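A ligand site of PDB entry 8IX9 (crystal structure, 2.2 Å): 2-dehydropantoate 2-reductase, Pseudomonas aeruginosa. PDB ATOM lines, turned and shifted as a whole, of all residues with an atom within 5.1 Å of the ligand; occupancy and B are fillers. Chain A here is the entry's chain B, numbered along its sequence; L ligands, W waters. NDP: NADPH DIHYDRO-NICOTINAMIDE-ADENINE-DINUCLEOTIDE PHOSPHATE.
The side-chain carboxylate (OE2) of Glu 278 is in hydrogen-bond range of the backbone NH (N) of Thr 83 (2.8 Å). The side-chain amino group (NZ) of Lys 196 lies within hydrogen-bond range of the side-chain amide oxygen (OD1) of Asn 108, at 3.1 Å. The side-chain amide nitrogen of Gln 107 is in hydrogen-bond range of the backbone carbonyl oxygen of Lys 82, 3.5 Å away. The side-chain carboxylate (OD1) of Asp 270 lies within salt-bridge range of the side-chain amino group (NZ) of Lys 82, at 2.6 Å. O of Cys 131 sits at hydrogen-bond distance from NZ of Lys 196 (3.1 Å). The backbone carbonyl oxygen (O) of Lys 196 lies close to the side-chain amide oxygen (OD1) of Asn 200 (3.4 Å). The backbone carbonyl oxygen (O) of Ala 81 is in hydrogen-bond range of the side-chain amide nitrogen (NE2) of Gln 107 (2.7 Å). The backbone carbonyl oxygen (O) of Leu 34 lies within hydrogen-bond range of the side-chain hydroxyl (OG1) of Thr 13 (2.7 Å).
The backbone carbonyl oxygen (O) of Leu 106 lies close to an oxygen (O4D) of the ligand. Residues that only touch the ligand: Leu 92, Lys 196, Ala 81, Gly 80, Tyr 263, Gly 12, Gln 107, Thr 13, Leu 89 and Glu 38. Hydrophobic or aromatic side chains that line the ligand: Ala 15, Ile 16, Ala 81, Leu 89 and Leu 92. Of the 34 residues printed, 24 come within 4 Å of the ligand. The nearest printed residue that does not touch the ligand is Leu 35 (4.003 Å).
Water W9 lies within hydrogen-bond range of the backbone NH of Thr 13 (2.6 Å), a nitrogen (N3A) of the ligand (2.8 Å) and the backbone carbonyl oxygen of Leu 34 (3.1 Å). Water W7 lies within hydrogen-bond range of an oxygen (O2A) of the ligand (2.9 Å) and the backbone NH of Arg 137 (3.1 Å). Water W6 bridges the backbone NH of Lys 82 (3.0 Å) and an oxygen (O4B) of the ligand (3.5 Å). Water W1 lies within hydrogen-bond range of O of Leu 106, O4D of the ligand and SG of Cys 131.
An oxygen (O2X) of the ligand is in hydrogen-bond range of the backbone NH of Ser 37. The side-chain hydroxyl of Ser 37 lies within hydrogen-bond range of an oxygen (O2X) of the ligand, at 2.6 Å. The side-chain carboxylate (OE1) of Glu 278 lies within hydrogen-bond range of an oxygen (O2D) of the ligand (2.6 Å). NH1 of Arg 137 is in salt-bridge range of O3X of the ligand, 2.7 Å away. O of Ile 133 sits at hydrogen-bond distance from N7N of the ligand, at 2.7 Å. O3D of the ligand is in hydrogen-bond range of N of Asn 108. The side-chain amide nitrogen (ND2) of Asn 108 is in hydrogen-bond range of an oxygen (O2D) of the ligand, at 2.8 Å. The backbone NH (N) of Ile 16 lies within hydrogen-bond range of an oxygen (O1N) of the ligand (2.8 Å). The guanidinium group of Arg 36 is in salt-bridge range of an oxygen (O1X) of the ligand, 2.9 Å away. NZ of Lys 82 lies within salt-bridge range of O1A of the ligand, at 3.0 Å. The backbone NH (N) of Gly 14 is in hydrogen-bond range of an oxygen (O3B) of the ligand. An oxygen (O1N) of the ligand sits at hydrogen-bond distance from the backbone NH (N) of Ala 15. O of Cys 131 sits at hydrogen-bond distance from N7N of the ligand, 3.4 Å away. O2D of the ligand lies within hydrogen-bond range of OG of Ser 266 (3.5 Å). ND2 of Asn 200 lies within hydrogen-bond range of O7N of the ligand (3.5 Å).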
ATOM      1  N   GLY A  12      -9.255 -10.905 -10.724  1.00  0.00           N
ATOM      2  CA  GLY A  12      -8.829 -10.350 -12.003  1.00  0.00           C
ATOM      3  C   GLY A  12     -10.018 -10.184 -12.924  1.00  0.00           C
ATOM      4  O   GLY A  12     -10.392 -11.107 -13.657  1.00  0.00           O
ATOM      5  N   THR A  13     -10.634  -9.000 -12.901  1.00  0.00           N
ATOM      6  CA  THR A  13     -11.899  -8.762 -13.596  1.00  0.00           C
ATOM      7  C   THR A  13     -11.661  -7.961 -14.863  1.00  0.00           C
ATOM      8  O   THR A  13     -12.013  -6.788 -14.991  1.00  0.00           O
ATOM      9  CB  THR A  13     -12.890  -8.075 -12.666  1.00  0.00           C
ATOM     10  OG1 THR A  13     -12.939  -8.775 -11.415  1.00  0.00           O
ATOM     11  CG2 THR A  13     -14.284  -8.062 -13.273  1.00  0.00           C
ATOM     12  N   GLY A  14     -11.038  -8.621 -15.821  1.00  0.00           N
ATOM     13  CA  GLY A  14     -10.845  -8.101 -17.162  1.00  0.00           C
ATOM     14  C   GLY A  14     -11.867  -8.646 -18.131  1.00  0.00           C
ATOM     15  O   GLY A  14     -13.014  -8.934 -17.769  1.00  0.00           O
ATOM     16  N   ALA A  15     -11.454  -8.800 -19.389  1.00  0.00           N
ATOM     17  CA  ALA A  15     -12.357  -9.292 -20.419  1.00  0.00           C
ATOM     18  C   ALA A  15     -12.883 -10.681 -20.062  1.00  0.00           C
ATOM     19  O   ALA A  15     -14.098 -10.924 -20.103  1.00  0.00           O
ATOM     20  CB  ALA A  15     -11.651  -9.317 -21.773  1.00  0.00           C
ATOM     21  N   ILE A  16     -11.981 -11.590 -19.696  1.00  0.00           N
ATOM     22  CA  ILE A  16     -12.392 -12.960 -19.386  1.00  0.00           C
ATOM     23  C   ILE A  16     -13.123 -13.026 -18.055  1.00  0.00           C
ATOM     24  O   ILE A  16     -14.220 -13.580 -17.961  1.00  0.00           O
ATOM     25  CB  ILE A  16     -11.167 -13.896 -19.393  1.00  0.00           C
ATOM     26  CG1 ILE A  16     -10.647 -14.065 -20.820  1.00  0.00           C
ATOM     27  CG2 ILE A  16     -11.528 -15.243 -18.803  1.00  0.00           C
ATOM     28  CD1 ILE A  16     -11.491 -14.974 -21.678  1.00  0.00           C
ATOM     29  N   GLY A  17     -12.518 -12.458 -17.010  1.00  0.00           N
ATOM     30  CA  GLY A  17     -13.149 -12.491 -15.695  1.00  0.00           C
ATOM     31  C   GLY A  17     -14.473 -11.755 -15.673  1.00  0.00           C
ATOM     32  O   GLY A  17     -15.451 -12.232 -15.083  1.00  0.00           O
ATOM     33  N   LEU A  34     -13.086  -8.990  -7.720  1.00  0.00           N
ATOM     34  CA  LEU A  34     -11.897  -8.228  -7.335  1.00  0.00           C
ATOM     35  C   LEU A  34     -11.384  -7.462  -8.556  1.00  0.00           C
ATOM     36  O   LEU A  34     -11.072  -8.076  -9.584  1.00  0.00           O
ATOM     37  CB  LEU A  34     -10.800  -9.136  -6.777  1.00  0.00           C
ATOM     38  CG  LEU A  34      -9.483  -8.415  -6.437  1.00  0.00           C
ATOM     39  CD1 LEU A  34      -9.673  -7.405  -5.317  1.00  0.00           C
ATOM     40  CD2 LEU A  34      -8.380  -9.407  -6.098  1.00  0.00           C
ATOM     41  N   LEU A  35     -11.310  -6.148  -8.439  1.00  0.00           N
ATOM     42  CA  LEU A  35     -10.850  -5.285  -9.515  1.00  0.00           C
ATOM     43  C   LEU A  35      -9.612  -4.523  -9.078  1.00  0.00           C
ATOM     44  O   LEU A  35      -9.296  -4.434  -7.891  1.00  0.00           O
ATOM     45  CB  LEU A  35     -11.951  -4.305  -9.947  1.00  0.00           C
ATOM     46  CG  LEU A  35     -13.237  -4.947 -10.486  1.00  0.00           C
ATOM     47  CD1 LEU A  35     -14.424  -4.578  -9.615  1.00  0.00           C
ATOM     48  CD2 LEU A  35     -13.479  -4.541 -11.927  1.00  0.00           C
ATOM     49  N   ARG A  36      -8.898  -3.967 -10.069  1.00  0.00           N
ATOM     50  CA  ARG A  36      -7.726  -3.160  -9.787  1.00  0.00           C
ATOM     51  C   ARG A  36      -7.942  -1.795 -10.441  1.00  0.00           C
ATOM     52  O   ARG A  36      -8.671  -0.965  -9.875  1.00  0.00           O
ATOM     53  CB  ARG A  36      -6.449  -3.861 -10.265  1.00  0.00           C
ATOM     54  CG  ARG A  36      -5.171  -3.207  -9.767  1.00  0.00           C
ATOM     55  CD  ARG A  36      -3.952  -4.095  -9.984  1.00  0.00           C
ATOM     56  NE  ARG A  36      -3.823  -4.523 -11.381  1.00  0.00           N
ATOM     57  CZ  ARG A  36      -2.869  -5.347 -11.822  1.00  0.00           C
ATOM     58  NH1 ARG A  36      -1.950  -5.818 -11.001  1.00  0.00           N
ATOM     59  NH2 ARG A  36      -2.834  -5.678 -13.104  1.00  0.00           N
ATOM     60  N   SER A  37      -7.359  -1.538 -11.603  1.00  0.00           N
ATOM     61  CA  SER A  37      -7.362  -0.188 -12.174  1.00  0.00           C
ATOM     62  C   SER A  37      -8.771   0.327 -12.447  1.00  0.00           C
ATOM     63  O   SER A  37      -9.031   1.526 -12.313  1.00  0.00           O
ATOM     64  CB  SER A  37      -6.535  -0.150 -13.454  1.00  0.00           C
ATOM     65  OG  SER A  37      -7.063  -1.037 -14.424  1.00  0.00           O
ATOM     66  N   GLU A  38      -9.693  -0.565 -12.811  1.00  0.00           N
ATOM     67  CA  GLU A  38     -11.042  -0.150 -13.174  1.00  0.00           C
ATOM     68  C   GLU A  38     -12.028  -0.310 -12.018  1.00  0.00           C
ATOM     69  O   GLU A  38     -13.244  -0.326 -12.262  1.00  0.00           O
ATOM     70  CB  GLU A  38     -11.519  -0.937 -14.387  1.00  0.00           C
ATOM     71  CG  GLU A  38     -10.546  -0.884 -15.561  1.00  0.00           C
ATOM     72  CD  GLU A  38     -10.924  -1.839 -16.673  1.00  0.00           C
ATOM     73  OE1 GLU A  38     -11.541  -1.386 -17.671  1.00  0.00           O
ATOM     74  OE2 GLU A  38     -10.608  -3.043 -16.556  1.00  0.00           O
ATOM     75  N   GLY A  80      -9.106 -14.575 -13.651  1.00  0.00           N
ATOM     76  CA  GLY A  80      -9.081 -13.962 -14.962  1.00  0.00           C
ATOM     77  C   GLY A  80      -7.926 -13.021 -15.198  1.00  0.00           C
ATOM     78  O   GLY A  80      -7.949 -12.272 -16.176  1.00  0.00           O
ATOM     79  N   ALA A  81      -6.927 -12.999 -14.325  1.00  0.00           N
ATOM     80  CA  ALA A  81      -5.730 -12.230 -14.610  1.00  0.00           C
ATOM     81  C   ALA A  81      -4.947 -12.880 -15.729  1.00  0.00           C
ATOM     82  O   ALA A  81      -5.119 -14.060 -16.048  1.00  0.00           O
ATOM     83  CB  ALA A  81      -4.855 -12.101 -13.355  1.00  0.00           C
ATOM     84  N   LYS A  82      -4.076 -12.098 -16.355  1.00  0.00           N
ATOM     85  CA  LYS A  82      -3.113 -12.690 -17.262  1.00  0.00           C
ATOM     86  C   LYS A  82      -2.113 -13.522 -16.468  1.00  0.00           C
ATOM     87  O   LYS A  82      -1.933 -13.329 -15.260  1.00  0.00           O
ATOM     88  CB  LYS A  82      -2.416 -11.607 -18.095  1.00  0.00           C
ATOM     89  CG  LYS A  82      -3.374 -10.787 -18.965  1.00  0.00           C
ATOM     90  CD  LYS A  82      -3.090 -10.981 -20.453  1.00  0.00           C
ATOM     91  CE  LYS A  82      -4.181 -10.410 -21.349  1.00  0.00           C
ATOM     92  NZ  LYS A  82      -4.294  -8.918 -21.281  1.00  0.00           N
ATOM     93  N   THR A  83      -1.478 -14.487 -17.138  1.00  0.00           N
ATOM     94  CA  THR A  83      -0.566 -15.379 -16.444  1.00  0.00           C
ATOM     95  C   THR A  83       0.690 -14.680 -15.949  1.00  0.00           C
ATOM     96  O   THR A  83       1.371 -15.208 -15.069  1.00  0.00           O
ATOM     97  CB  THR A  83      -0.161 -16.554 -17.334  1.00  0.00           C
ATOM     98  OG1 THR A  83       0.414 -16.052 -18.554  1.00  0.00           O
ATOM     99  CG2 THR A  83      -1.361 -17.429 -17.659  1.00  0.00           C
ATOM    100  N   LEU A  89      -0.395 -13.119  -7.691  1.00  0.00           N
ATOM    101  CA  LEU A  89      -1.824 -13.352  -7.516  1.00  0.00           C
ATOM    102  C   LEU A  89      -2.120 -14.346  -6.408  1.00  0.00           C
ATOM    103  O   LEU A  89      -3.201 -14.278  -5.800  1.00  0.00           O
ATOM    104  CB  LEU A  89      -2.433 -13.846  -8.827  1.00  0.00           C
ATOM    105  CG  LEU A  89      -3.907 -13.487  -8.979  1.00  0.00           C
ATOM    106  CD1 LEU A  89      -4.102 -11.988  -8.802  1.00  0.00           C
ATOM    107  CD2 LEU A  89      -4.404 -13.922 -10.329  1.00  0.00           C
ATOM    108  N   LEU A  92      -3.661 -13.393  -3.089  1.00  0.00           N
ATOM    109  CA  LEU A  92      -5.034 -12.930  -3.233  1.00  0.00           C
ATOM    110  C   LEU A  92      -6.001 -14.099  -3.343  1.00  0.00           C
ATOM    111  O   LEU A  92      -7.095 -14.065  -2.756  1.00  0.00           O
ATOM    112  CB  LEU A  92      -5.151 -12.031  -4.470  1.00  0.00           C
ATOM    113  CG  LEU A  92      -4.101 -10.911  -4.586  1.00  0.00           C
ATOM    114  CD1 LEU A  92      -4.435 -10.011  -5.756  1.00  0.00           C
ATOM    115  CD2 LEU A  92      -4.021 -10.116  -3.300  1.00  0.00           C
ATOM    116  N   LEU A 106      -8.765 -19.310 -15.716  1.00  0.00           N
ATOM    117  CA  LEU A 106      -9.254 -19.009 -17.056  1.00  0.00           C
ATOM    118  C   LEU A 106      -8.130 -18.324 -17.844  1.00  0.00           C
ATOM    119  O   LEU A 106      -8.185 -17.145 -18.197  1.00  0.00           O
ATOM    120  CB  LEU A 106     -10.503 -18.140 -16.972  1.00  0.00           C
ATOM    121  CG  LEU A 106     -11.584 -18.737 -16.071  1.00  0.00           C
ATOM    122  CD1 LEU A 106     -12.774 -17.793 -15.918  1.00  0.00           C
ATOM    123  CD2 LEU A 106     -12.024 -20.084 -16.626  1.00  0.00           C
ATOM    124  N   GLN A 107      -7.090 -19.114 -18.128  1.00  0.00           N
ATOM    125  CA  GLN A 107      -5.830 -18.581 -18.611  1.00  0.00           C
ATOM    126  C   GLN A 107      -5.271 -19.459 -19.716  1.00  0.00           C
ATOM    127  O   GLN A 107      -5.412 -20.680 -19.685  1.00  0.00           O
ATOM    128  CB  GLN A 107      -4.829 -18.457 -17.455  1.00  0.00           C
ATOM    129  CG  GLN A 107      -5.217 -17.407 -16.410  1.00  0.00           C
ATOM    130  CD  GLN A 107      -4.259 -17.351 -15.231  1.00  0.00           C
ATOM    131  OE1 GLN A 107      -3.821 -18.373 -14.713  1.00  0.00           O
ATOM    132  NE2 GLN A 107      -3.938 -16.135 -14.798  1.00  0.00           N
ATOM    133  N   ASN A 108      -4.620 -18.819 -20.689  1.00  0.00           N
ATOM    134  CA  ASN A 108      -3.948 -19.528 -21.769  1.00  0.00           C
ATOM    135  C   ASN A 108      -2.574 -20.017 -21.306  1.00  0.00           C
ATOM    136  O   ASN A 108      -2.094 -19.679 -20.223  1.00  0.00           O
ATOM    137  CB  ASN A 108      -3.785 -18.617 -22.994  1.00  0.00           C
ATOM    138  CG  ASN A 108      -5.060 -18.498 -23.800  1.00  0.00           C
ATOM    139  OD1 ASN A 108      -5.892 -19.412 -23.827  1.00  0.00           O
ATOM    140  ND2 ASN A 108      -5.218 -17.375 -24.487  1.00  0.00           N
ATOM    141  N   CYS A 131     -10.837 -21.345 -22.266  1.00  0.00           N
ATOM    142  CA  CYS A 131     -11.969 -20.577 -22.791  1.00  0.00           C
ATOM    143  C   CYS A 131     -11.750 -20.299 -24.269  1.00  0.00           C
ATOM    144  O   CYS A 131     -10.754 -19.677 -24.654  1.00  0.00           O
ATOM    145  CB  CYS A 131     -12.151 -19.271 -22.027  1.00  0.00           C
ATOM    146  SG  CYS A 131     -12.180 -19.444 -20.237  1.00  0.00           S
ATOM    147  N   PHE A 132     -12.695 -20.739 -25.091  1.00  0.00           N
ATOM    148  CA  PHE A 132     -12.659 -20.530 -26.538  1.00  0.00           C
ATOM    149  C   PHE A 132     -13.673 -19.431 -26.824  1.00  0.00           C
ATOM    150  O   PHE A 132     -14.875 -19.686 -26.925  1.00  0.00           O
ATOM    151  CB  PHE A 132     -12.944 -21.835 -27.272  1.00  0.00           C
ATOM    152  CG  PHE A 132     -12.041 -22.960 -26.832  1.00  0.00           C
ATOM    153  CD1 PHE A 132     -10.887 -23.248 -27.545  1.00  0.00           C
ATOM    154  CD2 PHE A 132     -12.319 -23.699 -25.692  1.00  0.00           C
ATOM    155  CE1 PHE A 132     -10.046 -24.263 -27.143  1.00  0.00           C
ATOM    156  CE2 PHE A 132     -11.477 -24.714 -25.290  1.00  0.00           C
ATOM    157  CZ  PHE A 132     -10.333 -24.994 -26.009  1.00  0.00           C
ATOM    158  N   ILE A 133     -13.177 -18.200 -26.929  1.00  0.00           N
ATOM    159  CA  ILE A 133     -14.024 -17.005 -26.873  1.00  0.00           C
ATOM    160  C   ILE A 133     -13.258 -15.854 -27.526  1.00  0.00           C
ATOM    161  O   ILE A 133     -12.046 -15.736 -27.384  1.00  0.00           O
ATOM    162  CB  ILE A 133     -14.411 -16.683 -25.410  1.00  0.00           C
ATOM    163  CG1 ILE A 133     -15.326 -15.458 -25.345  1.00  0.00           C
ATOM    164  CG2 ILE A 133     -13.168 -16.470 -24.547  1.00  0.00           C
ATOM    165  CD1 ILE A 133     -15.811 -15.150 -23.936  1.00  0.00           C
ATOM    166  N   CYS A 134     -13.999 -15.021 -28.262  1.00  0.00           N
ATOM    167  CA  CYS A 134     -13.485 -13.767 -28.803  1.00  0.00           C
ATOM    168  C   CYS A 134     -14.064 -12.642 -27.961  1.00  0.00           C
ATOM    169  O   CYS A 134     -15.236 -12.275 -28.111  1.00  0.00           O
ATOM    170  CB  CYS A 134     -13.837 -13.612 -30.280  1.00  0.00           C
ATOM    171  SG  CYS A 134     -13.174 -14.889 -31.368  1.00  0.00           S
ATOM    172  N   VAL A 135     -13.251 -12.093 -27.061  1.00  0.00           N
ATOM    173  CA  VAL A 135     -13.719 -11.079 -26.116  1.00  0.00           C
ATOM    174  C   VAL A 135     -12.565 -10.133 -25.803  1.00  0.00           C
ATOM    175  O   VAL A 135     -11.399 -10.530 -25.811  1.00  0.00           O
ATOM    176  CB  VAL A 135     -14.293 -11.732 -24.839  1.00  0.00           C
ATOM    177  CG1 VAL A 135     -13.177 -12.353 -24.005  1.00  0.00           C
ATOM    178  CG2 VAL A 135     -15.083 -10.722 -24.015  1.00  0.00           C
ATOM    179  N   ARG A 137     -11.874  -6.030 -23.573  1.00  0.00           N
ATOM    180  CA  ARG A 137     -12.421  -4.918 -22.828  1.00  0.00           C
ATOM    181  C   ARG A 137     -12.638  -3.729 -23.761  1.00  0.00           C
ATOM    182  O   ARG A 137     -11.766  -3.413 -24.575  1.00  0.00           O
ATOM    183  CB  ARG A 137     -11.498  -4.524 -21.671  1.00  0.00           C
ATOM    184  CG  ARG A 137     -11.708  -5.347 -20.415  1.00  0.00           C
ATOM    185  CD  ARG A 137     -10.861  -4.829 -19.264  1.00  0.00           C
ATOM    186  NE  ARG A 137      -9.429  -4.944 -19.536  1.00  0.00           N
ATOM    187  CZ  ARG A 137      -8.469  -4.531 -18.723  1.00  0.00           C
ATOM    188  NH1 ARG A 137      -8.778  -3.980 -17.556  1.00  0.00           N
ATOM    189  NH2 ARG A 137      -7.190  -4.676 -19.058  1.00  0.00           N
ATOM    190  N   LYS A 196      -4.951 -26.245 -27.177  1.00  0.00           N
ATOM    191  CA  LYS A 196      -5.236 -24.824 -27.264  1.00  0.00           C
ATOM    192  C   LYS A 196      -4.026 -24.034 -27.743  1.00  0.00           C
ATOM    193  O   LYS A 196      -4.183 -22.969 -28.368  1.00  0.00           O
ATOM    194  CB  LYS A 196      -5.719 -24.322 -25.909  1.00  0.00           C
ATOM    195  CG  LYS A 196      -5.896 -22.824 -25.784  1.00  0.00           C
ATOM    196  CD  LYS A 196      -7.166 -22.378 -26.467  1.00  0.00           C
ATOM    197  CE  LYS A 196      -7.737 -21.142 -25.791  1.00  0.00           C
ATOM    198  NZ  LYS A 196      -8.153 -21.431 -24.392  1.00  0.00           N
ATOM    199  N   ASN A 200      -3.259 -20.468 -30.108  1.00  0.00           N
ATOM    200  CA  ASN A 200      -2.739 -19.261 -29.484  1.00  0.00           C
ATOM    201  C   ASN A 200      -1.298 -18.973 -29.892  1.00  0.00           C
ATOM    202  O   ASN A 200      -0.908 -17.797 -29.967  1.00  0.00           O
ATOM    203  CB  ASN A 200      -2.849 -19.351 -27.966  1.00  0.00           C
ATOM    204  CG  ASN A 200      -4.257 -19.059 -27.474  1.00  0.00           C
ATOM    205  OD1 ASN A 200      -4.969 -19.946 -27.020  1.00  0.00           O
ATOM    206  ND2 ASN A 200      -4.664 -17.791 -27.562  1.00  0.00           N
ATOM    207  N   TYR A 263     -10.843 -10.597 -35.394  1.00  0.00           N
ATOM    208  CA  TYR A 263     -10.580 -10.597 -33.963  1.00  0.00           C
ATOM    209  C   TYR A 263      -9.132 -10.240 -33.678  1.00  0.00           C
ATOM    210  O   TYR A 263      -8.219 -10.721 -34.353  1.00  0.00           O
ATOM    211  CB  TYR A 263     -10.915 -11.957 -33.369  1.00  0.00           C
ATOM    212  CG  TYR A 263     -10.483 -12.159 -31.924  1.00  0.00           C
ATOM    213  CD1 TYR A 263     -11.142 -11.505 -30.891  1.00  0.00           C
ATOM    214  CD2 TYR A 263      -9.448 -13.013 -31.606  1.00  0.00           C
ATOM    215  CE1 TYR A 263     -10.772 -11.693 -29.581  1.00  0.00           C
ATOM    216  CE2 TYR A 263      -9.068 -13.208 -30.291  1.00  0.00           C
ATOM    217  CZ  TYR A 263      -9.725 -12.542 -29.278  1.00  0.00           C
ATOM    218  OH  TYR A 263      -9.355 -12.730 -27.969  1.00  0.00           O
ATOM    219  N   SER A 266      -5.735 -11.432 -27.470  1.00  0.00           N
ATOM    220  CA  SER A 266      -5.427 -10.752 -26.215  1.00  0.00           C
ATOM    221  C   SER A 266      -4.026 -10.153 -26.240  1.00  0.00           C
ATOM    222  O   SER A 266      -3.811  -9.036 -25.765  1.00  0.00           O
ATOM    223  CB  SER A 266      -5.576 -11.727 -25.052  1.00  0.00           C
ATOM    224  OG  SER A 266      -4.656 -12.798 -25.182  1.00  0.00           O
ATOM    225  N   ASP A 270      -2.362  -6.336 -25.387  1.00  0.00           N
ATOM    226  CA  ASP A 270      -1.296  -6.145 -24.420  1.00  0.00           C
ATOM    227  C   ASP A 270      -0.181  -5.272 -24.983  1.00  0.00           C
ATOM    228  O   ASP A 270       0.276  -4.327 -24.336  1.00  0.00           O
ATOM    229  CB  ASP A 270      -0.734  -7.490 -23.975  1.00  0.00           C
ATOM    230  CG  ASP A 270      -1.597  -8.170 -22.931  1.00  0.00           C
ATOM    231  OD1 ASP A 270      -2.373  -7.459 -22.245  1.00  0.00           O
ATOM    232  OD2 ASP A 270      -1.508  -9.404 -22.791  1.00  0.00           O
ATOM    233  N   ARG A 275       1.408  -3.392 -22.006  1.00  0.00           N
ATOM    234  CA  ARG A 275       1.400  -4.406 -20.982  1.00  0.00           C
ATOM    235  C   ARG A 275       2.322  -5.559 -21.372  1.00  0.00           C
ATOM    236  O   ARG A 275       2.493  -5.846 -22.560  1.00  0.00           O
ATOM    237  CB  ARG A 275      -0.010  -4.942 -20.760  1.00  0.00           C
ATOM    238  CG  ARG A 275      -1.025  -3.870 -20.364  1.00  0.00           C
ATOM    239  CD  ARG A 275      -2.359  -4.480 -19.977  1.00  0.00           C
ATOM    240  NE  ARG A 275      -3.010  -5.161 -21.094  1.00  0.00           N
ATOM    241  CZ  ARG A 275      -4.082  -4.690 -21.734  1.00  0.00           C
ATOM    242  NH1 ARG A 275      -4.621  -3.533 -21.372  1.00  0.00           N
ATOM    243  NH2 ARG A 275      -4.610  -5.374 -22.744  1.00  0.00           N
ATOM    244  N   GLU A 278       2.269 -12.382 -22.524  1.00  0.00           N
ATOM    245  CA  GLU A 278       2.236 -13.696 -21.891  1.00  0.00           C
ATOM    246  C   GLU A 278       3.202 -14.653 -22.575  1.00  0.00           C
ATOM    247  O   GLU A 278       2.828 -15.788 -22.905  1.00  0.00           O
ATOM    248  CB  GLU A 278       0.819 -14.264 -21.919  1.00  0.00           C
ATOM    249  CG  GLU A 278      -0.211 -13.459 -21.165  1.00  0.00           C
ATOM    250  CD  GLU A 278      -1.547 -14.172 -21.060  1.00  0.00           C
ATOM    251  OE1 GLU A 278      -2.233 -14.314 -22.096  1.00  0.00           O
ATOM    252  OE2 GLU A 278      -1.920 -14.591 -19.943  1.00  0.00           O
ATOM    253  N   ILE A 282       2.891 -19.007 -22.958  1.00  0.00           N
ATOM    254  CA  ILE A 282       2.471 -19.399 -24.299  1.00  0.00           C
ATOM    255  C   ILE A 282       3.628 -19.861 -25.171  1.00  0.00           C
ATOM    256  O   ILE A 282       3.457 -20.755 -26.011  1.00  0.00           O
ATOM    257  CB  ILE A 282       1.685 -18.261 -24.958  1.00  0.00           C
ATOM    258  CG1 ILE A 282       0.385 -17.991 -24.194  1.00  0.00           C
ATOM    259  CG2 ILE A 282       1.351 -18.584 -26.419  1.00  0.00           C
ATOM    260  CD1 ILE A 282      -0.383 -16.788 -24.688  1.00  0.00           C
HETATM  261  PA  NDP L   1      -7.351  -8.440 -19.435  1.00  0.00           P
HETATM  262  O1A NDP L   1      -6.169  -7.517 -19.369  1.00  0.00           O
HETATM  263  O2A NDP L   1      -8.422  -7.838 -20.253  1.00  0.00           O
HETATM  264  O5B NDP L   1      -7.913  -8.745 -17.892  1.00  0.00           O
HETATM  265  C5B NDP L   1      -7.004  -9.189 -16.926  1.00  0.00           C
HETATM  266  C4B NDP L   1      -7.505  -8.660 -15.589  1.00  0.00           C
HETATM  267  O4B NDP L   1      -6.819  -9.174 -14.609  1.00  0.00           O
HETATM  268  C3B NDP L   1      -7.234  -7.122 -15.547  1.00  0.00           C
HETATM  269  O3B NDP L   1      -8.421  -6.446 -15.309  1.00  0.00           O
HETATM  270  C2B NDP L   1      -6.284  -6.951 -14.390  1.00  0.00           C
HETATM  271  O2B NDP L   1      -6.516  -5.632 -13.711  1.00  0.00           O
HETATM  272  C1B NDP L   1      -6.593  -7.975 -13.589  1.00  0.00           C
HETATM  273  N9A NDP L   1      -5.465  -8.249 -12.724  1.00  0.00           N
HETATM  274  C8A NDP L   1      -4.207  -8.705 -12.823  1.00  0.00           C
HETATM  275  N7A NDP L   1      -3.673  -8.709 -11.601  1.00  0.00           N
HETATM  276  C5A NDP L   1      -4.603  -8.260 -10.740  1.00  0.00           C
HETATM  277  C6A NDP L   1      -4.570  -8.073  -9.374  1.00  0.00           C
HETATM  278  N6A NDP L   1      -3.567  -8.274  -8.334  1.00  0.00           N
HETATM  279  N1A NDP L   1      -5.638  -7.606  -8.732  1.00  0.00           N
HETATM  280  C2A NDP L   1      -6.764  -7.314  -9.432  1.00  0.00           C
HETATM  281  N3A NDP L   1      -6.789  -7.500 -10.779  1.00  0.00           N
HETATM  282  C4A NDP L   1      -5.711  -7.974 -11.429  1.00  0.00           C
HETATM  283  O3  NDP L   1      -6.893  -9.880 -20.094  1.00  0.00           O
HETATM  284  PN  NDP L   1      -7.967 -11.047 -20.613  1.00  0.00           P
HETATM  285  O1N NDP L   1      -9.198 -11.045 -19.777  1.00  0.00           O
HETATM  286  O2N NDP L   1      -8.316 -10.812 -22.022  1.00  0.00           O
HETATM  287  O5D NDP L   1      -7.222 -12.506 -20.507  1.00  0.00           O
HETATM  288  C5D NDP L   1      -6.978 -13.160 -19.236  1.00  0.00           C
HETATM  289  C4D NDP L   1      -6.517 -14.644 -19.621  1.00  0.00           C
HETATM  290  O4D NDP L   1      -7.401 -15.172 -20.412  1.00  0.00           O
HETATM  291  C3D NDP L   1      -5.217 -14.574 -20.431  1.00  0.00           C
HETATM  292  O3D NDP L   1      -4.392 -15.643 -20.072  1.00  0.00           O
HETATM  293  C2D NDP L   1      -5.657 -14.700 -21.885  1.00  0.00           C
HETATM  294  O2D NDP L   1      -4.547 -15.293 -22.744  1.00  0.00           O
HETATM  295  C1D NDP L   1      -6.705 -15.489 -21.816  1.00  0.00           C
HETATM  296  N1N NDP L   1      -7.652 -15.232 -22.937  1.00  0.00           N
HETATM  297  C2N NDP L   1      -8.105 -16.321 -23.720  1.00  0.00           C
HETATM  298  C3N NDP L   1      -8.942 -16.158 -24.943  1.00  0.00           C
HETATM  299  C7N NDP L   1      -8.821 -17.203 -26.037  1.00  0.00           C
HETATM  300  O7N NDP L   1      -7.836 -17.914 -26.091  1.00  0.00           O
HETATM  301  N7N NDP L   1      -9.851 -17.342 -26.998  1.00  0.00           N
HETATM  302  C4N NDP L   1      -9.559 -14.762 -25.323  1.00  0.00           C
HETATM  303  C5N NDP L   1      -9.175 -13.627 -24.331  1.00  0.00           C
HETATM  304  C6N NDP L   1      -8.124 -13.884 -23.207  1.00  0.00           C
HETATM  305  P2B NDP L   1      -5.998  -4.251 -14.495  1.00  0.00           P
HETATM  306  O1X NDP L   1      -4.659  -4.472 -15.083  1.00  0.00           O
HETATM  307  O2X NDP L   1      -5.915  -3.139 -13.457  1.00  0.00           O
HETATM  308  O3X NDP L   1      -6.960  -3.878 -15.552  1.00  0.00           O
HETATM  309  O   HOH W   1      -8.910 -17.751 -20.940  1.00  0.00           O
HETATM  310  O   HOH W   2      -9.974 -11.113 -17.109  1.00  0.00           O
HETATM  311  O   HOH W   3      -4.026  -7.024 -17.822  1.00  0.00           O
HETATM  312  O   HOH W   4      -8.202  -9.203 -24.352  1.00  0.00           O
HETATM  313  O   HOH W   5      -2.987  -1.925 -13.719  1.00  0.00           O
HETATM  314  O   HOH W   6      -3.512  -9.213 -15.663  1.00  0.00           O
HETATM  315  O   HOH W   7      -9.020  -6.953 -22.912  1.00  0.00           O
HETATM  316  O   HOH W   8      -5.641  -6.456  -5.880  1.00  0.00           O
HETATM  317  O   HOH W   9      -9.322  -6.991 -11.938  1.00  0.00           O
